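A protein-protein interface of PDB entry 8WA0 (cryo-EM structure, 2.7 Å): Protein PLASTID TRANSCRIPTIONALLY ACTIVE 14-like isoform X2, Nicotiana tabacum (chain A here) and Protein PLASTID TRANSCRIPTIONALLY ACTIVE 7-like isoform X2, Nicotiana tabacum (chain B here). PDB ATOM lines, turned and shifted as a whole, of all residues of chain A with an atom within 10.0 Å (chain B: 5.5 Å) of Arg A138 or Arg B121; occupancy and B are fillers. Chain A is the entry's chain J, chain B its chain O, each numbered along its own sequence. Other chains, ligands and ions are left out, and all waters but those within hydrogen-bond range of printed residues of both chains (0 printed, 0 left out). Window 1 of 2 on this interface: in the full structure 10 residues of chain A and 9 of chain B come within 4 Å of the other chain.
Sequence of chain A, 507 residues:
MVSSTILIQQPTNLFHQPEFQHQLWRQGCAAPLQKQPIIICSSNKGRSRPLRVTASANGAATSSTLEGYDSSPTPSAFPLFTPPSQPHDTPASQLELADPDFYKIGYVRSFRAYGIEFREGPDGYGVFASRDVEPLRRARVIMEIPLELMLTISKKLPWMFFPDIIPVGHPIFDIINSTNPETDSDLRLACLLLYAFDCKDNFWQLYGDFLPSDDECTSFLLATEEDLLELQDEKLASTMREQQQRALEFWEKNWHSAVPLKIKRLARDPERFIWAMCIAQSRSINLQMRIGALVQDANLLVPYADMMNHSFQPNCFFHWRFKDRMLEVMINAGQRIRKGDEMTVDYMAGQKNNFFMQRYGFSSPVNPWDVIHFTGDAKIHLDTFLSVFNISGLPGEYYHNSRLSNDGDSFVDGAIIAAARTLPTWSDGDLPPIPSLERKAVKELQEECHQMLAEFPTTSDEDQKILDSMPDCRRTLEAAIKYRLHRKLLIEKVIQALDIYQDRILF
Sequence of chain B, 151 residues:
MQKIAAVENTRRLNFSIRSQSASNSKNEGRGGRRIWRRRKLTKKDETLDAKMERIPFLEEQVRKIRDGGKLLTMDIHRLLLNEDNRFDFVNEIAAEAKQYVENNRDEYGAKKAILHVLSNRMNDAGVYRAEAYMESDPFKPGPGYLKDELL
NH2 of Arg A137 is in salt-bridge range of OE2 of Glu B96 (3.8 Å). NH2 of Arg A140 lies within hydrogen-bond range of O of Asp B124, 2.9 Å away.
Leu A136 touches Asp B124 (CD1 to O, 3.7 Å). Arg A137 touches Asp B124 (CD to OD2, 3.3 Å). NH2 of Arg A138 touches NE of Arg B121, 3.8 Å away. C of Ala B125 touches NE of Arg A140, at 3.9 Å.
O of Leu A136 lies within hydrogen-bond range of N of Gly A334, at 3.2 Å. The backbone carbonyl oxygen of Arg A140 sits at hydrogen-bond distance from the backbone NH of Ile A331 (3.0 Å). The side-chain carboxylate (OE2) of Glu B92 is in salt-bridge range of the guanidinium group (NH2) of Arg B121 (2.7 Å). OE1 of Glu B96 lies within salt-bridge range of NH2 of Arg B121.
Of the 15 printed residues of chain B, 4 touch a printed residue of chain A. Of the 16 printed residues of chain A, 4 touch a printed residue of chain B. Printed residues of chain A that touch a printed residue of chain B: Leu A136, Arg A137, Arg A138 and Arg A140. Hydrophobic or aromatic side chains of chain A that line the printed part of chain B: Leu A136. Among the printed residues, 6 pairs touch across the chains.
Printed residues of chain B within 4 Å of Leu A136: Asp B124. Of the printed residues of chain A, Glu B96 touches Arg A137. Arg B121 touches one residue of chain A. Asp B124 touches just these residues of chain A: Leu A136 (3.7 Å), Arg A137 (3.3 Å) and Arg A140 (2.9 Å). Printed residues of chain A within 4 Å of Ala B125: Arg A140 (3.9 Å). The nearest residue of chain B that does not touch Arg A138 is Glu B92 (4.1 Å).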
ATOM      1  N   VAL A 133      -9.668  23.749  -2.434  1.00  0.00           N
ATOM      2  CA  VAL A 133      -9.682  23.637  -1.019  1.00  0.00           C
ATOM      3  C   VAL A 133     -10.428  22.363  -0.717  1.00  0.00           C
ATOM      4  O   VAL A 133     -11.526  22.188  -1.159  1.00  0.00           O
ATOM      5  CB  VAL A 133     -10.465  24.814  -0.454  1.00  0.00           C
ATOM      6  CG1 VAL A 133     -10.613  24.704   1.047  1.00  0.00           C
ATOM      7  CG2 VAL A 133      -9.818  26.133  -0.832  1.00  0.00           C
ATOM      8  N   GLU A 134      -9.844  21.475   0.051  1.00  0.00           N
ATOM      9  CA  GLU A 134     -10.440  20.227   0.408  1.00  0.00           C
ATOM     10  C   GLU A 134     -11.356  20.436   1.574  1.00  0.00           C
ATOM     11  O   GLU A 134     -11.385  21.520   2.128  1.00  0.00           O
ATOM     12  CB  GLU A 134      -9.314  19.264   0.715  1.00  0.00           C
ATOM     13  CG  GLU A 134      -8.379  19.740   1.810  1.00  0.00           C
ATOM     14  CD  GLU A 134      -8.389  18.827   3.019  1.00  0.00           C
ATOM     15  OE1 GLU A 134      -8.978  17.730   2.930  1.00  0.00           O
ATOM     16  OE2 GLU A 134      -7.809  19.206   4.058  1.00  0.00           O
ATOM     17  N   PRO A 135     -12.152  19.439   1.943  1.00  0.00           N
ATOM     18  CA  PRO A 135     -13.068  19.706   3.014  1.00  0.00           C
ATOM     19  C   PRO A 135     -12.221  20.088   4.186  1.00  0.00           C
ATOM     20  O   PRO A 135     -11.229  19.421   4.420  1.00  0.00           O
ATOM     21  CB  PRO A 135     -13.684  18.362   3.220  1.00  0.00           C
ATOM     22  CG  PRO A 135     -13.679  17.724   1.894  1.00  0.00           C
ATOM     23  CD  PRO A 135     -12.336  18.090   1.389  1.00  0.00           C
ATOM     24  N   LEU A 136     -12.584  21.101   4.950  1.00  0.00           N
ATOM     25  CA  LEU A 136     -11.722  21.607   6.001  1.00  0.00           C
ATOM     26  C   LEU A 136     -12.285  21.601   7.383  1.00  0.00           C
ATOM     27  O   LEU A 136     -13.462  21.711   7.566  1.00  0.00           O
ATOM     28  CB  LEU A 136     -11.362  23.031   5.661  1.00  0.00           C
ATOM     29  CG  LEU A 136     -10.297  23.380   4.636  1.00  0.00           C
ATOM     30  CD1 LEU A 136     -10.161  24.890   4.608  1.00  0.00           C
ATOM     31  CD2 LEU A 136      -8.973  22.733   5.003  1.00  0.00           C
ATOM     32  N   ARG A 137     -11.451  21.460   8.379  1.00  0.00           N
ATOM     33  CA  ARG A 137     -11.881  21.445   9.755  1.00  0.00           C
ATOM     34  C   ARG A 137     -12.472  22.701  10.324  1.00  0.00           C
ATOM     35  O   ARG A 137     -13.415  22.637  11.072  1.00  0.00           O
ATOM     36  CB  ARG A 137     -10.673  21.080  10.574  1.00  0.00           C
ATOM     37  CG  ARG A 137      -9.840  19.965   9.970  1.00  0.00           C
ATOM     38  CD  ARG A 137      -8.493  19.851  10.661  1.00  0.00           C
ATOM     39  NE  ARG A 137      -8.631  19.762  12.112  1.00  0.00           N
ATOM     40  CZ  ARG A 137      -8.715  18.622  12.790  1.00  0.00           C
ATOM     41  NH1 ARG A 137      -8.669  17.460  12.152  1.00  0.00           N
ATOM     42  NH2 ARG A 137      -8.842  18.643  14.110  1.00  0.00           N
ATOM     43  N   ARG A 138     -11.913  23.843  10.005  1.00  0.00           N
ATOM     44  CA  ARG A 138     -12.378  25.113  10.491  1.00  0.00           C
ATOM     45  C   ARG A 138     -12.362  26.052   9.322  1.00  0.00           C
ATOM     46  O   ARG A 138     -11.792  25.722   8.302  1.00  0.00           O
ATOM     47  CB  ARG A 138     -11.451  25.627  11.568  1.00  0.00           C
ATOM     48  CG  ARG A 138     -12.027  25.583  12.965  1.00  0.00           C
ATOM     49  CD  ARG A 138     -10.944  25.893  13.977  1.00  0.00           C
ATOM     50  NE  ARG A 138      -9.888  24.898  13.926  1.00  0.00           N
ATOM     51  CZ  ARG A 138      -9.778  23.881  14.766  1.00  0.00           C
ATOM     52  NH1 ARG A 138     -10.653  23.728  15.739  1.00  0.00           N
ATOM     53  NH2 ARG A 138      -8.783  23.024  14.638  1.00  0.00           N
ATOM     54  N   ALA A 139     -12.956  27.210   9.436  1.00  0.00           N
ATOM     55  CA  ALA A 139     -13.029  28.192   8.391  1.00  0.00           C
ATOM     56  C   ALA A 139     -11.790  28.825   7.841  1.00  0.00           C
ATOM     57  O   ALA A 139     -10.828  28.991   8.561  1.00  0.00           O
ATOM     58  CB  ALA A 139     -13.816  29.288   8.980  1.00  0.00           C
ATOM     59  N   ARG A 140     -11.783  29.208   6.576  1.00  0.00           N
ATOM     60  CA  ARG A 140     -10.659  29.867   5.949  1.00  0.00           C
ATOM     61  C   ARG A 140     -10.952  31.230   5.386  1.00  0.00           C
ATOM     62  O   ARG A 140     -11.897  31.394   4.681  1.00  0.00           O
ATOM     63  CB  ARG A 140     -10.094  29.046   4.825  1.00  0.00           C
ATOM     64  CG  ARG A 140      -8.896  29.662   4.151  1.00  0.00           C
ATOM     65  CD  ARG A 140      -8.448  28.866   2.952  1.00  0.00           C
ATOM     66  NE  ARG A 140      -7.895  27.593   3.349  1.00  0.00           N
ATOM     67  CZ  ARG A 140      -7.187  26.814   2.553  1.00  0.00           C
ATOM     68  NH1 ARG A 140      -6.931  27.193   1.316  1.00  0.00           N
ATOM     69  NH2 ARG A 140      -6.723  25.663   3.000  1.00  0.00           N
ATOM     70  N   VAL A 141     -10.126  32.222   5.652  1.00  0.00           N
ATOM     71  CA  VAL A 141     -10.349  33.556   5.172  1.00  0.00           C
ATOM     72  C   VAL A 141     -10.070  33.799   3.716  1.00  0.00           C
ATOM     73  O   VAL A 141      -8.995  33.487   3.243  1.00  0.00           O
ATOM     74  CB  VAL A 141      -9.497  34.541   5.957  1.00  0.00           C
ATOM     75  CG1 VAL A 141      -9.975  35.961   5.751  1.00  0.00           C
ATOM     76  CG2 VAL A 141      -9.517  34.191   7.429  1.00  0.00           C
ATOM     77  N   PHE A 317     -19.424  33.252   4.462  1.00  0.00           N
ATOM     78  CA  PHE A 317     -20.055  34.094   5.481  1.00  0.00           C
ATOM     79  C   PHE A 317     -19.251  35.304   5.945  1.00  0.00           C
ATOM     80  O   PHE A 317     -18.101  35.415   5.595  1.00  0.00           O
ATOM     81  CB  PHE A 317     -20.552  33.251   6.662  1.00  0.00           C
ATOM     82  CG  PHE A 317     -19.513  32.829   7.648  1.00  0.00           C
ATOM     83  CD1 PHE A 317     -18.740  31.732   7.419  1.00  0.00           C
ATOM     84  CD2 PHE A 317     -19.394  33.474   8.857  1.00  0.00           C
ATOM     85  CE1 PHE A 317     -17.817  31.311   8.337  1.00  0.00           C
ATOM     86  CE2 PHE A 317     -18.472  33.063   9.784  1.00  0.00           C
ATOM     87  CZ  PHE A 317     -17.680  31.981   9.519  1.00  0.00           C
ATOM     88  N   MET A 330     -15.380  34.636   5.011  1.00  0.00           N
ATOM     89  CA  MET A 330     -14.844  33.346   5.234  1.00  0.00           C
ATOM     90  C   MET A 330     -15.548  32.150   4.625  1.00  0.00           C
ATOM     91  O   MET A 330     -16.754  32.127   4.640  1.00  0.00           O
ATOM     92  CB  MET A 330     -14.755  33.193   6.731  1.00  0.00           C
ATOM     93  CG  MET A 330     -13.897  34.176   7.457  1.00  0.00           C
ATOM     94  SD  MET A 330     -13.208  33.290   8.831  1.00  0.00           S
ATOM     95  CE  MET A 330     -14.540  33.383  10.014  1.00  0.00           C
ATOM     96  N   ILE A 331     -14.838  31.149   4.095  1.00  0.00           N
ATOM     97  CA  ILE A 331     -15.421  29.888   3.583  1.00  0.00           C
ATOM     98  C   ILE A 331     -15.964  28.951   4.654  1.00  0.00           C
ATOM     99  O   ILE A 331     -15.292  28.710   5.632  1.00  0.00           O
ATOM    100  CB  ILE A 331     -14.439  29.085   2.726  1.00  0.00           C
ATOM    101  CG1 ILE A 331     -13.695  29.970   1.750  1.00  0.00           C
ATOM    102  CG2 ILE A 331     -15.158  27.994   1.956  1.00  0.00           C
ATOM    103  CD1 ILE A 331     -12.746  29.191   0.875  1.00  0.00           C
ATOM    104  N   ASN A 332     -17.166  28.414   4.478  1.00  0.00           N
ATOM    105  CA  ASN A 332     -17.840  27.590   5.462  1.00  0.00           C
ATOM    106  C   ASN A 332     -17.130  26.321   5.709  1.00  0.00           C
ATOM    107  O   ASN A 332     -16.490  25.793   4.818  1.00  0.00           O
ATOM    108  CB  ASN A 332     -19.242  27.311   4.988  1.00  0.00           C
ATOM    109  CG  ASN A 332     -20.105  28.532   4.938  1.00  0.00           C
ATOM    110  OD1 ASN A 332     -19.688  29.626   5.306  1.00  0.00           O
ATOM    111  ND2 ASN A 332     -21.328  28.356   4.473  1.00  0.00           N
ATOM    112  N   ALA A 333     -17.215  25.810   6.921  1.00  0.00           N
ATOM    113  CA  ALA A 333     -16.491  24.619   7.267  1.00  0.00           C
ATOM    114  C   ALA A 333     -17.049  23.408   6.624  1.00  0.00           C
ATOM    115  O   ALA A 333     -18.256  23.234   6.561  1.00  0.00           O
ATOM    116  CB  ALA A 333     -16.499  24.432   8.742  1.00  0.00           C
ATOM    117  N   GLY A 334     -16.185  22.546   6.156  1.00  0.00           N
ATOM    118  CA  GLY A 334     -16.634  21.326   5.563  1.00  0.00           C
ATOM    119  C   GLY A 334     -17.045  21.269   4.129  1.00  0.00           C
ATOM    120  O   GLY A 334     -17.563  20.256   3.710  1.00  0.00           O
ATOM    121  N   GLN A 335     -16.825  22.315   3.356  1.00  0.00           N
ATOM    122  CA  GLN A 335     -17.305  22.323   1.992  1.00  0.00           C
ATOM    123  C   GLN A 335     -16.195  22.312   0.999  1.00  0.00           C
ATOM    124  O   GLN A 335     -15.285  23.116   1.084  1.00  0.00           O
ATOM    125  CB  GLN A 335     -18.239  23.503   1.768  1.00  0.00           C
ATOM    126  CG  GLN A 335     -19.040  23.437   0.495  1.00  0.00           C
ATOM    127  CD  GLN A 335     -20.127  24.475   0.474  1.00  0.00           C
ATOM    128  OE1 GLN A 335     -20.299  25.218   1.433  1.00  0.00           O
ATOM    129  NE2 GLN A 335     -20.876  24.530  -0.618  1.00  0.00           N
ATOM    130  N   LEU B  79      -2.816  33.827  15.469  1.00  0.00           N
ATOM    131  CA  LEU B  79      -3.825  32.996  16.031  1.00  0.00           C
ATOM    132  C   LEU B  79      -4.501  33.528  17.227  1.00  0.00           C
ATOM    133  O   LEU B  79      -5.609  33.144  17.508  1.00  0.00           O
ATOM    134  CB  LEU B  79      -3.222  31.632  16.256  1.00  0.00           C
ATOM    135  CG  LEU B  79      -2.813  30.764  15.090  1.00  0.00           C
ATOM    136  CD1 LEU B  79      -2.219  29.482  15.621  1.00  0.00           C
ATOM    137  CD2 LEU B  79      -3.997  30.476  14.193  1.00  0.00           C
ATOM    138  N   PHE B  89      -7.511  29.628  24.965  1.00  0.00           N
ATOM    139  CA  PHE B  89      -6.767  29.119  23.854  1.00  0.00           C
ATOM    140  C   PHE B  89      -5.623  28.257  24.295  1.00  0.00           C
ATOM    141  O   PHE B  89      -5.368  27.246  23.673  1.00  0.00           O
ATOM    142  CB  PHE B  89      -6.379  30.284  22.993  1.00  0.00           C
ATOM    143  CG  PHE B  89      -5.749  29.948  21.689  1.00  0.00           C
ATOM    144  CD1 PHE B  89      -6.487  29.410  20.666  1.00  0.00           C
ATOM    145  CD2 PHE B  89      -4.429  30.263  21.458  1.00  0.00           C
ATOM    146  CE1 PHE B  89      -5.907  29.138  19.452  1.00  0.00           C
ATOM    147  CE2 PHE B  89      -3.842  29.997  20.250  1.00  0.00           C
ATOM    148  CZ  PHE B  89      -4.583  29.432  19.245  1.00  0.00           C
ATOM    149  N   GLU B  92      -7.284  24.965  25.041  1.00  0.00           N
ATOM    150  CA  GLU B  92      -7.625  24.210  23.854  1.00  0.00           C
ATOM    151  C   GLU B  92      -6.468  23.529  23.174  1.00  0.00           C
ATOM    152  O   GLU B  92      -6.578  22.371  22.813  1.00  0.00           O
ATOM    153  CB  GLU B  92      -8.274  25.114  22.864  1.00  0.00           C
ATOM    154  CG  GLU B  92      -8.683  24.475  21.558  1.00  0.00           C
ATOM    155  CD  GLU B  92      -9.238  25.491  20.586  1.00  0.00           C
ATOM    156  OE1 GLU B  92      -9.420  26.655  20.993  1.00  0.00           O
ATOM    157  OE2 GLU B  92      -9.491  25.127  19.417  1.00  0.00           O
ATOM    158  N   ILE B  93      -5.349  24.184  23.011  1.00  0.00           N
ATOM    159  CA  ILE B  93      -4.159  23.603  22.432  1.00  0.00           C
ATOM    160  C   ILE B  93      -3.583  22.494  23.242  1.00  0.00           C
ATOM    161  O   ILE B  93      -3.175  21.477  22.697  1.00  0.00           O
ATOM    162  CB  ILE B  93      -3.122  24.667  22.025  1.00  0.00           C
ATOM    163  CG1 ILE B  93      -3.694  25.571  20.951  1.00  0.00           C
ATOM    164  CG2 ILE B  93      -1.819  24.054  21.554  1.00  0.00           C
ATOM    165  CD1 ILE B  93      -2.711  26.608  20.490  1.00  0.00           C
ATOM    166  N   GLU B  96      -5.636  19.270  22.526  1.00  0.00           N
ATOM    167  CA  GLU B  96      -5.362  18.644  21.267  1.00  0.00           C
ATOM    168  C   GLU B  96      -4.084  17.897  21.272  1.00  0.00           C
ATOM    169  O   GLU B  96      -3.996  16.836  20.686  1.00  0.00           O
ATOM    170  CB  GLU B  96      -5.398  19.634  20.149  1.00  0.00           C
ATOM    171  CG  GLU B  96      -5.901  19.088  18.840  1.00  0.00           C
ATOM    172  CD  GLU B  96      -6.152  20.186  17.837  1.00  0.00           C
ATOM    173  OE1 GLU B  96      -6.142  21.363  18.243  1.00  0.00           O
ATOM    174  OE2 GLU B  96      -6.364  19.875  16.647  1.00  0.00           O
ATOM    175  N   HIS B 116       3.121  20.356  16.376  1.00  0.00           N
ATOM    176  CA  HIS B 116       2.283  19.754  15.381  1.00  0.00           C
ATOM    177  C   HIS B 116       0.894  20.316  15.333  1.00  0.00           C
ATOM    178  O   HIS B 116       0.368  20.524  14.261  1.00  0.00           O
ATOM    179  CB  HIS B 116       2.250  18.277  15.608  1.00  0.00           C
ATOM    180  CG  HIS B 116       1.867  17.475  14.413  1.00  0.00           C
ATOM    181  ND1 HIS B 116       1.833  17.997  13.143  1.00  0.00           N
ATOM    182  CD2 HIS B 116       1.523  16.174  14.297  1.00  0.00           C
ATOM    183  CE1 HIS B 116       1.470  17.055  12.294  1.00  0.00           C
ATOM    184  NE2 HIS B 116       1.280  15.939  12.970  1.00  0.00           N
ATOM    185  N   VAL B 117       0.286  20.592  16.465  1.00  0.00           N
ATOM    186  CA  VAL B 117      -1.030  21.160  16.509  1.00  0.00           C
ATOM    187  C   VAL B 117      -1.019  22.500  15.871  1.00  0.00           C
ATOM    188  O   VAL B 117      -1.867  22.789  15.065  1.00  0.00           O
ATOM    189  CB  VAL B 117      -1.549  21.242  17.925  1.00  0.00           C
ATOM    190  CG1 VAL B 117      -2.808  22.071  18.017  1.00  0.00           C
ATOM    191  CG2 VAL B 117      -1.743  19.869  18.516  1.00  0.00           C
ATOM    192  N   LEU B 118      -0.033  23.314  16.168  1.00  0.00           N
ATOM    193  CA  LEU B 118       0.088  24.639  15.587  1.00  0.00           C
ATOM    194  C   LEU B 118       0.377  24.686  14.107  1.00  0.00           C
ATOM    195  O   LEU B 118      -0.183  25.519  13.417  1.00  0.00           O
ATOM    196  CB  LEU B 118       1.013  25.499  16.419  1.00  0.00           C
ATOM    197  CG  LEU B 118       0.628  25.955  17.813  1.00  0.00           C
ATOM    198  CD1 LEU B 118       1.865  26.337  18.595  1.00  0.00           C
ATOM    199  CD2 LEU B 118      -0.323  27.125  17.720  1.00  0.00           C
ATOM    200  N   SER B 119       1.228  23.818  13.588  1.00  0.00           N
ATOM    201  CA  SER B 119       1.476  23.743  12.169  1.00  0.00           C
ATOM    202  C   SER B 119       0.270  23.319  11.453  1.00  0.00           C
ATOM    203  O   SER B 119      -0.003  23.819  10.378  1.00  0.00           O
ATOM    204  CB  SER B 119       2.555  22.785  11.853  1.00  0.00           C
ATOM    205  OG  SER B 119       2.196  21.468  12.207  1.00  0.00           O
ATOM    206  N   ASN B 120      -0.475  22.383  12.002  1.00  0.00           N
ATOM    207  CA  ASN B 120      -1.712  21.937  11.410  1.00  0.00           C
ATOM    208  C   ASN B 120      -2.736  23.030  11.332  1.00  0.00           C
ATOM    209  O   ASN B 120      -3.416  23.135  10.340  1.00  0.00           O
ATOM    210  CB  ASN B 120      -2.208  20.648  11.997  1.00  0.00           C
ATOM    211  CG  ASN B 120      -1.453  19.456  11.511  1.00  0.00           C
ATOM    212  OD1 ASN B 120      -1.648  18.355  12.006  1.00  0.00           O
ATOM    213  ND2 ASN B 120      -0.587  19.659  10.534  1.00  0.00           N
ATOM    214  N   ARG B 121      -2.824  23.894  12.295  1.00  0.00           N
ATOM    215  CA  ARG B 121      -3.712  25.009  12.165  1.00  0.00           C
ATOM    216  C   ARG B 121      -3.355  25.940  11.042  1.00  0.00           C
ATOM    217  O   ARG B 121      -4.227  26.388  10.315  1.00  0.00           O
ATOM    218  CB  ARG B 121      -3.863  25.744  13.476  1.00  0.00           C
ATOM    219  CG  ARG B 121      -4.396  24.876  14.580  1.00  0.00           C
ATOM    220  CD  ARG B 121      -5.431  25.587  15.406  1.00  0.00           C
ATOM    221  NE  ARG B 121      -5.923  24.703  16.439  1.00  0.00           N
ATOM    222  CZ  ARG B 121      -6.827  25.040  17.337  1.00  0.00           C
ATOM    223  NH1 ARG B 121      -7.348  26.246  17.332  1.00  0.00           N
ATOM    224  NH2 ARG B 121      -7.207  24.162  18.239  1.00  0.00           N
ATOM    225  N   MET B 122      -2.100  26.234  10.865  1.00  0.00           N
ATOM    226  CA  MET B 122      -1.686  27.139   9.838  1.00  0.00           C
ATOM    227  C   MET B 122      -1.854  26.606   8.463  1.00  0.00           C
ATOM    228  O   MET B 122      -2.259  27.335   7.577  1.00  0.00           O
ATOM    229  CB  MET B 122      -0.286  27.654  10.103  1.00  0.00           C
ATOM    230  CG  MET B 122      -0.072  28.307  11.445  1.00  0.00           C
ATOM    231  SD  MET B 122      -0.699  29.981  11.516  1.00  0.00           S
ATOM    232  CE  MET B 122       0.184  30.726  10.156  1.00  0.00           C
ATOM    233  N   ASN B 123      -1.547  25.347   8.252  1.00  0.00           N
ATOM    234  CA  ASN B 123      -1.718  24.716   6.969  1.00  0.00           C
ATOM    235  C   ASN B 123      -3.166  24.632   6.562  1.00  0.00           C
ATOM    236  O   ASN B 123      -3.467  24.744   5.395  1.00  0.00           O
ATOM    237  CB  ASN B 123      -0.924  23.453   6.884  1.00  0.00           C
ATOM    238  CG  ASN B 123       0.558  23.698   6.918  1.00  0.00           C
ATOM    239  OD1 ASN B 123       1.020  24.675   7.487  1.00  0.00           O
ATOM    240  ND2 ASN B 123       1.314  22.801   6.327  1.00  0.00           N
ATOM    241  N   ASP B 124      -4.072  24.441   7.499  1.00  0.00           N
ATOM    242  CA  ASP B 124      -5.496  24.480   7.220  1.00  0.00           C
ATOM    243  C   ASP B 124      -5.951  25.821   6.732  1.00  0.00           C
ATOM    244  O   ASP B 124      -6.846  25.895   5.922  1.00  0.00           O
ATOM    245  CB  ASP B 124      -6.297  24.088   8.424  1.00  0.00           C
ATOM    246  CG  ASP B 124      -6.113  22.639   8.795  1.00  0.00           C
ATOM    247  OD1 ASP B 124      -5.712  21.843   7.921  1.00  0.00           O
ATOM    248  OD2 ASP B 124      -6.372  22.293   9.966  1.00  0.00           O
ATOM    249  N   ALA B 125      -5.371  26.884   7.229  1.00  0.00           N
ATOM    250  CA  ALA B 125      -5.721  28.219   6.809  1.00  0.00           C
ATOM    251  C   ALA B 125      -4.933  28.787   5.669  1.00  0.00           C
ATOM    252  O   ALA B 125      -5.073  29.951   5.367  1.00  0.00           O
ATOM    253  CB  ALA B 125      -5.699  29.154   7.945  1.00  0.00           C
